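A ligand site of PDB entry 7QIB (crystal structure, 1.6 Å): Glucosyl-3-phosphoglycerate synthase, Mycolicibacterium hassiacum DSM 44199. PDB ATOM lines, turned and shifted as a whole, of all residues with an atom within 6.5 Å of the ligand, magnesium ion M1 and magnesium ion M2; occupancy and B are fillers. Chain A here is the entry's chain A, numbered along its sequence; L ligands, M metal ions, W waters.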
ATOM      1  N   LEU A  46      -8.649  34.424  -8.562  1.00  0.00           N
ATOM      2  CA  LEU A  46      -7.436  33.949  -7.929  1.00  0.00           C
ATOM      3  C   LEU A  46      -7.481  32.431  -7.883  1.00  0.00           C
ATOM      4  O   LEU A  46      -8.314  31.870  -7.140  1.00  0.00           O
ATOM      5  CB  LEU A  46      -7.319  34.513  -6.505  1.00  0.00           C
ATOM      6  CG  LEU A  46      -6.797  35.930  -6.258  1.00  0.00           C
ATOM      7  CD1 LEU A  46      -7.329  36.941  -7.239  1.00  0.00           C
ATOM      8  CD2 LEU A  46      -7.083  36.379  -4.827  1.00  0.00           C
ATOM      9  N   PRO A  47      -6.649  31.705  -8.628  1.00  0.00           N
ATOM     10  CA  PRO A  47      -6.501  30.274  -8.378  1.00  0.00           C
ATOM     11  C   PRO A  47      -5.775  30.049  -7.068  1.00  0.00           C
ATOM     12  O   PRO A  47      -4.861  30.801  -6.722  1.00  0.00           O
ATOM     13  CB  PRO A  47      -5.665  29.796  -9.565  1.00  0.00           C
ATOM     14  CG  PRO A  47      -4.768  30.995  -9.839  1.00  0.00           C
ATOM     15  CD  PRO A  47      -5.675  32.195  -9.627  1.00  0.00           C
ATOM     16  N   ALA A  48      -6.168  29.012  -6.329  1.00  0.00           N
ATOM     17  CA  ALA A  48      -5.515  28.800  -5.048  1.00  0.00           C
ATOM     18  C   ALA A  48      -5.452  27.316  -4.679  1.00  0.00           C
ATOM     19  O   ALA A  48      -6.487  26.650  -4.604  1.00  0.00           O
ATOM     20  CB  ALA A  48      -6.231  29.570  -3.935  1.00  0.00           C
ATOM     21  N   LEU A  49      -4.249  26.846  -4.403  1.00  0.00           N
ATOM     22  CA  LEU A  49      -4.027  25.529  -3.803  1.00  0.00           C
ATOM     23  C   LEU A  49      -3.098  25.707  -2.601  1.00  0.00           C
ATOM     24  O   LEU A  49      -1.899  25.930  -2.767  1.00  0.00           O
ATOM     25  CB  LEU A  49      -3.427  24.547  -4.804  1.00  0.00           C
ATOM     26  CG  LEU A  49      -3.132  23.143  -4.287  1.00  0.00           C
ATOM     27  CD1 LEU A  49      -4.417  22.516  -3.725  1.00  0.00           C
ATOM     28  CD2 LEU A  49      -2.527  22.250  -5.378  1.00  0.00           C
ATOM     29  N   ASN A  50      -3.667  25.627  -1.392  1.00  0.00           N
ATOM     30  CA  ASN A  50      -2.900  25.673  -0.143  1.00  0.00           C
ATOM     31  C   ASN A  50      -2.055  26.949  -0.045  1.00  0.00           C
ATOM     32  O   ASN A  50      -0.828  26.926   0.034  1.00  0.00           O
ATOM     33  CB  ASN A  50      -2.037  24.424   0.026  1.00  0.00           C
ATOM     34  CG  ASN A  50      -2.876  23.172   0.144  1.00  0.00           C
ATOM     35  OD1 ASN A  50      -3.912  23.174   0.797  1.00  0.00           O
ATOM     36  ND2 ASN A  50      -2.447  22.092  -0.518  1.00  0.00           N
ATOM     37  N   GLU A  51      -2.759  28.084  -0.050  1.00  0.00           N
ATOM     38  CA  GLU A  51      -2.091  29.373   0.075  1.00  0.00           C
ATOM     39  C   GLU A  51      -2.586  30.141   1.287  1.00  0.00           C
ATOM     40  O   GLU A  51      -2.868  31.331   1.196  1.00  0.00           O
ATOM     41  CB  GLU A  51      -2.302  30.220  -1.186  1.00  0.00           C
ATOM     42  CG  GLU A  51      -1.921  29.503  -2.485  1.00  0.00           C
ATOM     43  CD  GLU A  51      -0.439  29.213  -2.605  1.00  0.00           C
ATOM     44  OE1 GLU A  51       0.362  29.649  -1.757  1.00  0.00           O
ATOM     45  OE2 GLU A  51      -0.062  28.539  -3.593  1.00  0.00           O
ATOM     46  N   LEU A  76     -10.890  30.570  -6.848  1.00  0.00           N
ATOM     47  CA  LEU A  76     -11.248  29.259  -7.381  1.00  0.00           C
ATOM     48  C   LEU A  76     -10.343  28.276  -6.664  1.00  0.00           C
ATOM     49  O   LEU A  76      -9.162  28.152  -6.983  1.00  0.00           O
ATOM     50  CB  LEU A  76     -11.042  29.218  -8.894  1.00  0.00           C
ATOM     51  CG  LEU A  76     -11.886  28.267  -9.761  1.00  0.00           C
ATOM     52  CD1 LEU A  76     -11.896  26.824  -9.221  1.00  0.00           C
ATOM     53  CD2 LEU A  76     -13.300  28.779  -9.930  1.00  0.00           C
ATOM     54  N   ASP A  77     -10.871  27.631  -5.614  1.00  0.00           N
ATOM     55  CA  ASP A  77     -10.044  26.727  -4.834  1.00  0.00           C
ATOM     56  C   ASP A  77      -9.808  25.423  -5.568  1.00  0.00           C
ATOM     57  O   ASP A  77     -10.723  24.838  -6.163  1.00  0.00           O
ATOM     58  CB  ASP A  77     -10.669  26.430  -3.471  1.00  0.00           C
ATOM     59  CG  ASP A  77      -9.705  25.662  -2.593  1.00  0.00           C
ATOM     60  OD1 ASP A  77      -8.770  26.296  -2.047  1.00  0.00           O
ATOM     61  OD2 ASP A  77      -9.840  24.429  -2.495  1.00  0.00           O
ATOM     62  N   SER A  78      -8.560  24.948  -5.494  1.00  0.00           N
ATOM     63  CA  SER A  78      -8.047  23.823  -6.262  1.00  0.00           C
ATOM     64  C   SER A  78      -7.942  22.552  -5.421  1.00  0.00           C
ATOM     65  O   SER A  78      -7.216  21.626  -5.792  1.00  0.00           O
ATOM     66  CB  SER A  78      -6.679  24.221  -6.840  1.00  0.00           C
ATOM     67  OG  SER A  78      -6.223  23.316  -7.832  1.00  0.00           O
ATOM     68  N   ARG A  98     -13.568  23.705  -7.694  1.00  0.00           N
ATOM     69  CA  ARG A  98     -13.522  23.240  -9.074  1.00  0.00           C
ATOM     70  C   ARG A  98     -14.797  22.484  -9.445  1.00  0.00           C
ATOM     71  O   ARG A  98     -15.308  22.618 -10.566  1.00  0.00           O
ATOM     72  CB  ARG A  98     -12.308  22.335  -9.287  1.00  0.00           C
ATOM     73  CG  ARG A  98     -10.973  23.058  -9.204  1.00  0.00           C
ATOM     74  CD  ARG A  98      -9.842  22.055  -9.186  1.00  0.00           C
ATOM     75  NE  ARG A  98      -9.943  21.151  -8.049  1.00  0.00           N
ATOM     76  CZ  ARG A  98      -9.210  20.052  -7.901  1.00  0.00           C
ATOM     77  NH1 ARG A  98      -8.240  19.763  -8.745  1.00  0.00           N
ATOM     78  NH2 ARG A  98      -9.463  19.231  -6.895  1.00  0.00           N
ATOM     79  N   PRO A 109      -5.689  17.469 -11.956  1.00  0.00           N
ATOM     80  CA  PRO A 109      -4.802  18.370 -11.202  1.00  0.00           C
ATOM     81  C   PRO A 109      -4.245  19.494 -12.069  1.00  0.00           C
ATOM     82  O   PRO A 109      -4.221  19.412 -13.294  1.00  0.00           O
ATOM     83  CB  PRO A 109      -3.677  17.459 -10.723  1.00  0.00           C
ATOM     84  CG  PRO A 109      -4.267  16.073 -10.754  1.00  0.00           C
ATOM     85  CD  PRO A 109      -5.194  16.077 -11.922  1.00  0.00           C
ATOM     86  N   GLY A 110      -3.802  20.552 -11.405  1.00  0.00           N
ATOM     87  CA  GLY A 110      -2.992  21.560 -12.069  1.00  0.00           C
ATOM     88  C   GLY A 110      -3.681  22.909 -12.166  1.00  0.00           C
ATOM     89  O   GLY A 110      -4.905  23.039 -12.069  1.00  0.00           O
ATOM     90  N   LYS A 111      -2.852  23.942 -12.369  1.00  0.00           N
ATOM     91  CA  LYS A 111      -3.356  25.308 -12.414  1.00  0.00           C
ATOM     92  C   LYS A 111      -4.228  25.552 -13.630  1.00  0.00           C
ATOM     93  O   LYS A 111      -5.227  26.285 -13.566  1.00  0.00           O
ATOM     94  CB  LYS A 111      -2.186  26.298 -12.410  1.00  0.00           C
ATOM     95  CG  LYS A 111      -2.645  27.739 -12.319  1.00  0.00           C
ATOM     96  CD  LYS A 111      -1.554  28.710 -12.725  1.00  0.00           C
ATOM     97  CE  LYS A 111      -2.002  30.137 -12.441  1.00  0.00           C
ATOM     98  NZ  LYS A 111      -1.041  31.179 -12.951  1.00  0.00           N
ATOM     99  N   GLY A 112      -3.857  24.970 -14.774  1.00  0.00           N
ATOM    100  CA  GLY A 112      -4.622  25.222 -15.991  1.00  0.00           C
ATOM    101  C   GLY A 112      -6.072  24.818 -15.843  1.00  0.00           C
ATOM    102  O   GLY A 112      -6.972  25.505 -16.351  1.00  0.00           O
ATOM    103  N   VAL A 114      -7.856  24.960 -13.152  1.00  0.00           N
ATOM    104  CA  VAL A 114      -8.529  25.941 -12.316  1.00  0.00           C
ATOM    105  C   VAL A 114      -8.927  27.168 -13.139  1.00  0.00           C
ATOM    106  O   VAL A 114     -10.043  27.676 -13.028  1.00  0.00           O
ATOM    107  CB  VAL A 114      -7.619  26.321 -11.137  1.00  0.00           C
ATOM    108  CG1 VAL A 114      -8.262  27.391 -10.274  1.00  0.00           C
ATOM    109  CG2 VAL A 114      -7.284  25.087 -10.314  1.00  0.00           C
ATOM    110  N   ILE A 130      -4.900  36.506 -11.103  1.00  0.00           N
ATOM    111  CA  ILE A 130      -3.818  36.914 -10.220  1.00  0.00           C
ATOM    112  C   ILE A 130      -3.497  35.743  -9.308  1.00  0.00           C
ATOM    113  O   ILE A 130      -4.388  35.122  -8.724  1.00  0.00           O
ATOM    114  CB  ILE A 130      -4.175  38.183  -9.413  1.00  0.00           C
ATOM    115  CG1 ILE A 130      -4.181  39.405 -10.342  1.00  0.00           C
ATOM    116  CG2 ILE A 130      -3.202  38.385  -8.275  1.00  0.00           C
ATOM    117  CD1 ILE A 130      -4.755  40.654  -9.716  1.00  0.00           C
ATOM    118  N   ASP A 131      -2.202  35.437  -9.180  1.00  0.00           N
ATOM    119  CA  ASP A 131      -1.812  34.302  -8.343  1.00  0.00           C
ATOM    120  C   ASP A 131      -2.088  34.617  -6.874  1.00  0.00           C
ATOM    121  O   ASP A 131      -1.922  35.740  -6.411  1.00  0.00           O
ATOM    122  CB  ASP A 131      -0.320  33.971  -8.531  1.00  0.00           C
ATOM    123  CG  ASP A 131      -0.039  33.138  -9.811  1.00  0.00           C
ATOM    124  OD1 ASP A 131      -0.969  32.659 -10.499  1.00  0.00           O
ATOM    125  OD2 ASP A 131       1.158  32.963 -10.130  1.00  0.00           O
ATOM    126  N   SER A 132      -2.530  33.602  -6.139  1.00  0.00           N
ATOM    127  CA  SER A 132      -2.850  33.765  -4.733  1.00  0.00           C
ATOM    128  C   SER A 132      -1.644  33.588  -3.815  1.00  0.00           C
ATOM    129  O   SER A 132      -1.773  33.774  -2.600  1.00  0.00           O
ATOM    130  CB  SER A 132      -3.970  32.795  -4.336  1.00  0.00           C
ATOM    131  OG  SER A 132      -3.611  31.440  -4.617  1.00  0.00           O
ATOM    132  N   ASP A 133      -0.470  33.223  -4.362  1.00  0.00           N
ATOM    133  CA  ASP A 133       0.727  33.037  -3.549  1.00  0.00           C
ATOM    134  C   ASP A 133       1.602  34.287  -3.487  1.00  0.00           C
ATOM    135  O   ASP A 133       2.724  34.205  -2.966  1.00  0.00           O
ATOM    136  CB  ASP A 133       1.528  31.832  -4.054  1.00  0.00           C
ATOM    137  CG  ASP A 133       2.126  32.035  -5.452  1.00  0.00           C
ATOM    138  OD1 ASP A 133       1.841  33.048  -6.123  1.00  0.00           O
ATOM    139  OD2 ASP A 133       2.903  31.151  -5.872  1.00  0.00           O
ATOM    140  N   LEU A 134       1.128  35.430  -3.965  1.00  0.00           N
ATOM    141  CA  LEU A 134       1.939  36.632  -3.976  1.00  0.00           C
ATOM    142  C   LEU A 134       2.171  37.163  -2.559  1.00  0.00           C
ATOM    143  O   LEU A 134       1.225  37.339  -1.784  1.00  0.00           O
ATOM    144  CB  LEU A 134       1.278  37.706  -4.838  1.00  0.00           C
ATOM    145  CG  LEU A 134       1.055  37.294  -6.289  1.00  0.00           C
ATOM    146  CD1 LEU A 134       0.395  38.441  -7.039  1.00  0.00           C
ATOM    147  CD2 LEU A 134       2.378  36.928  -6.938  1.00  0.00           C
ATOM    148  N   GLY A 222      -1.856  22.346 -15.987  1.00  0.00           N
ATOM    149  CA  GLY A 222      -0.738  22.555 -15.067  1.00  0.00           C
ATOM    150  C   GLY A 222       0.069  23.792 -15.379  1.00  0.00           C
ATOM    151  O   GLY A 222      -0.475  24.888 -15.593  1.00  0.00           O
ATOM    152  N   TYR A 223       1.391  23.620 -15.399  1.00  0.00           N
ATOM    153  CA  TYR A 223       2.323  24.709 -15.644  1.00  0.00           C
ATOM    154  C   TYR A 223       2.291  25.215 -17.079  1.00  0.00           C
ATOM    155  O   TYR A 223       2.969  26.213 -17.375  1.00  0.00           O
ATOM    156  CB  TYR A 223       3.764  24.259 -15.350  1.00  0.00           C
ATOM    157  CG  TYR A 223       4.094  24.014 -13.896  1.00  0.00           C
ATOM    158  CD1 TYR A 223       4.030  25.051 -12.973  1.00  0.00           C
ATOM    159  CD2 TYR A 223       4.537  22.767 -13.472  1.00  0.00           C
ATOM    160  CE1 TYR A 223       4.363  24.840 -11.649  1.00  0.00           C
ATOM    161  CE2 TYR A 223       4.867  22.547 -12.143  1.00  0.00           C
ATOM    162  CZ  TYR A 223       4.777  23.582 -11.237  1.00  0.00           C
ATOM    163  OH  TYR A 223       5.109  23.370  -9.913  1.00  0.00           O
ATOM    164  N   ASP A 259      11.166  21.504  -8.867  1.00  0.00           N
ATOM    165  CA  ASP A 259       9.968  22.207  -9.335  1.00  0.00           C
ATOM    166  C   ASP A 259      10.214  22.881 -10.676  1.00  0.00           C
ATOM    167  O   ASP A 259       9.372  22.801 -11.574  1.00  0.00           O
ATOM    168  CB  ASP A 259       9.528  23.239  -8.296  1.00  0.00           C
ATOM    169  CG  ASP A 259       8.713  22.629  -7.166  1.00  0.00           C
ATOM    170  OD1 ASP A 259       8.601  21.392  -7.108  1.00  0.00           O
ATOM    171  OD2 ASP A 259       8.184  23.408  -6.333  1.00  0.00           O
ATOM    172  N   MET A 263       8.281  22.266 -14.268  1.00  0.00           N
ATOM    173  CA  MET A 263       7.668  23.388 -14.977  1.00  0.00           C
ATOM    174  C   MET A 263       8.199  23.457 -16.395  1.00  0.00           C
ATOM    175  O   MET A 263       7.436  23.632 -17.346  1.00  0.00           O
ATOM    176  CB  MET A 263       7.963  24.685 -14.224  1.00  0.00           C
ATOM    177  CG  MET A 263       7.369  25.935 -14.862  1.00  0.00           C
ATOM    178  SD  MET A 263       7.890  27.420 -13.980  1.00  0.00           S
ATOM    179  CE  MET A 263       8.123  26.735 -12.330  1.00  0.00           C
HETATM  180  N1  LIG L   1      -2.380  26.629  -8.148  1.00  0.00           N
HETATM  181  C1  LIG L   1      -3.658  26.103  -8.166  1.00  0.00           C
HETATM  182  N2  LIG L   1      -3.734  24.764  -8.470  1.00  0.00           N
HETATM  183  C2  LIG L   1      -2.673  23.919  -8.750  1.00  0.00           C
HETATM  184  C3  LIG L   1      -1.389  24.553  -8.725  1.00  0.00           C
HETATM  185  C4  LIG L   1      -1.282  25.858  -8.427  1.00  0.00           C
HETATM  186  O1  LIG L   1      -4.666  26.769  -7.930  1.00  0.00           O
HETATM  187  O2  LIG L   1      -2.891  22.726  -9.003  1.00  0.00           O
HETATM  188  C5  LIG L   1      -2.225  28.070  -7.837  1.00  0.00           C
HETATM  189  C6  LIG L   1      -1.263  28.341  -6.684  1.00  0.00           C
HETATM  190  O3  LIG L   1      -1.974  28.338  -5.442  1.00  0.00           O
HETATM  191  C7  LIG L   1      -0.716  29.725  -7.038  1.00  0.00           C
HETATM  192  C8  LIG L   1      -0.702  29.709  -8.572  1.00  0.00           C
HETATM  193  O4  LIG L   1      -1.661  28.707  -8.969  1.00  0.00           O
HETATM  194  O5  LIG L   1      -1.558  30.787  -6.601  1.00  0.00           O
HETATM  195  C9  LIG L   1       0.639  29.411  -9.198  1.00  0.00           C
HETATM  196  O6  LIG L   1       1.060  28.126  -8.683  1.00  0.00           O
HETATM  197  P1  LIG L   1       2.580  27.695  -8.657  1.00  0.00           P
HETATM  198  O7  LIG L   1       3.046  27.658 -10.063  1.00  0.00           O
HETATM  199  O8  LIG L   1       3.377  28.548  -7.669  1.00  0.00           O
HETATM  200  O9  LIG L   1       2.549  26.244  -8.056  1.00  0.00           O
HETATM  201  P2  LIG L   1       3.787  25.460  -7.442  1.00  0.00           P
HETATM  202  O10 LIG L   1       4.911  25.307  -8.436  1.00  0.00           O
HETATM  203  O11 LIG L   1       3.165  24.141  -7.004  1.00  0.00           O
HETATM  204  O12 LIG L   1       4.149  26.307  -6.221  1.00  0.00           O
HETATM  205 MG    MG M   1       1.479  27.146  -3.630  1.00  0.00          MG
HETATM  206 MG    MG M   2       4.159  30.676  -7.476  1.00  0.00          MG
HETATM  207  O   HOH W   1       3.295  26.005  -3.673  1.00  0.00           O
HETATM  208  O   HOH W   2       3.153  32.375  -8.168  1.00  0.00           O
HETATM  209  O   HOH W   3       0.093  25.659  -4.703  1.00  0.00           O
HETATM  210  O   HOH W   4       1.079  23.492  -5.576  1.00  0.00           O
HETATM  211  O   HOH W   5      -0.645  21.015  -8.331  1.00  0.00           O
HETATM  212  O   HOH W   6       1.083  26.097  -1.784  1.00  0.00           O
HETATM  213  O   HOH W   7       1.076  26.530 -11.753  1.00  0.00           O
HETATM  214  O   HOH W   8       2.300  28.209  -5.124  1.00  0.00           O
HETATM  215  O   HOH W   9       1.613  22.770  -9.647  1.00  0.00           O
HETATM  216  O   HOH W  10       4.088  29.575  -4.213  1.00  0.00           O
HETATM  217  O   HOH W  11       2.546  28.708  -2.269  1.00  0.00           O
HETATM  218  O   HOH W  12      -4.701  20.783  -8.462  1.00  0.00           O
HETATM  219  O   HOH W  13       5.242  32.112  -6.551  1.00  0.00           O
HETATM  220  O   HOH W  14       5.400  29.386  -6.632  1.00  0.00           O
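Magnesium ion M2 is bound by water W14 (2.0 Å), water W13 (2.0 Å), OD2 of Asp 133 (2.1 Å), water W2 (2.1 Å) and O8 of the ligand (2.3 Å). Magnesium ion M2 has five donor atoms within binding distance.
O3 of the ligand sits close to OE2 of Glu 51 (2.7 Å). O5 of the ligand is in hydrogen-bond range of N of Asp 133 (3.5 Å). OH of Tyr 223 lies within hydrogen-bond range of O10 of the ligand, at 2.4 Å. N of Leu 49 is in hydrogen-bond range of O3 of the ligand (2.9 Å). The backbone NH (N) of Ser 132 is in hydrogen-bond range of an oxygen (O5) of the ligand (3.0 Å). The side-chain hydroxyl (OG) of Ser 132 lies within hydrogen-bond range of an oxygen (O5) of the ligand (2.9 Å). A nitrogen (N2) of the ligand lies within hydrogen-bond range of the side-chain hydroxyl (OG) of Ser 78 (2.9 Å). O1 of the ligand is in hydrogen-bond range of N of Ala 48 (3.1 Å). An oxygen (O2) of the ligand lies close to the backbone NH (N) of Gly 110, at 3.4 Å. O of Pro 47 lies within hydrogen-bond range of O5 of the ligand (3.3 Å).
Water W3 bridges the backbone carbonyl oxygen (O) of Leu 49 and an oxygen (O3) of the ligand. Water W2 lies within hydrogen-bond range of the side-chain carboxylate (OD1) of Asp 133 (2.5 Å) and the side-chain carboxylate (OD2) of Asp 131 (2.9 Å). Water W12 lies within hydrogen-bond range of an oxygen (O2) of the ligand (2.7 Å), the side-chain hydroxyl of Ser 78 (3.0 Å) and the backbone NH of Gly 110 (3.1 Å).
Merely in contact with the ligand: Asp 131 (3.5 Å), Lys 111 (3.6 Å) and Val 114 (3.9 Å). Hydrophobic or aromatic side chains that line the ligand: Pro 47, Leu 49, Val 114 and Tyr 223. Of the 24 residues printed, 12 come within 4 Å of the ligand.
The side-chain hydroxyl (OG) of Ser 132 is in hydrogen-bond range of the backbone carbonyl oxygen (O) of Pro 47. The backbone carbonyl oxygen (O) of Ala 48 is in hydrogen-bond range of the backbone NH (N) of Ser 78 (2.8 Å). The backbone carbonyl oxygen of Ser 78 lies close to the guanidinium group of Arg 98 (3.5 Å). The backbone carbonyl oxygen (O) of Leu 76 is in hydrogen-bond range of the backbone NH (N) of Ala 48, 3.2 Å away. The side-chain amino group (NZ) of Lys 111 is in salt-bridge range of the side-chain carboxylate (OD1) of Asp 131.
Leu 49 touches magnesium ion M1. Within 4 Å of magnesium ion M1: Leu 49 and Glu 51.
Magnesium ion M1 is bound by water W8 (2.0 Å), OE2 of Glu 51 (2.1 Å), water W1 (2.1 Å), water W6 (2.2 Å), water W3 (2.3 Å) and water W11 (2.3 Å).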
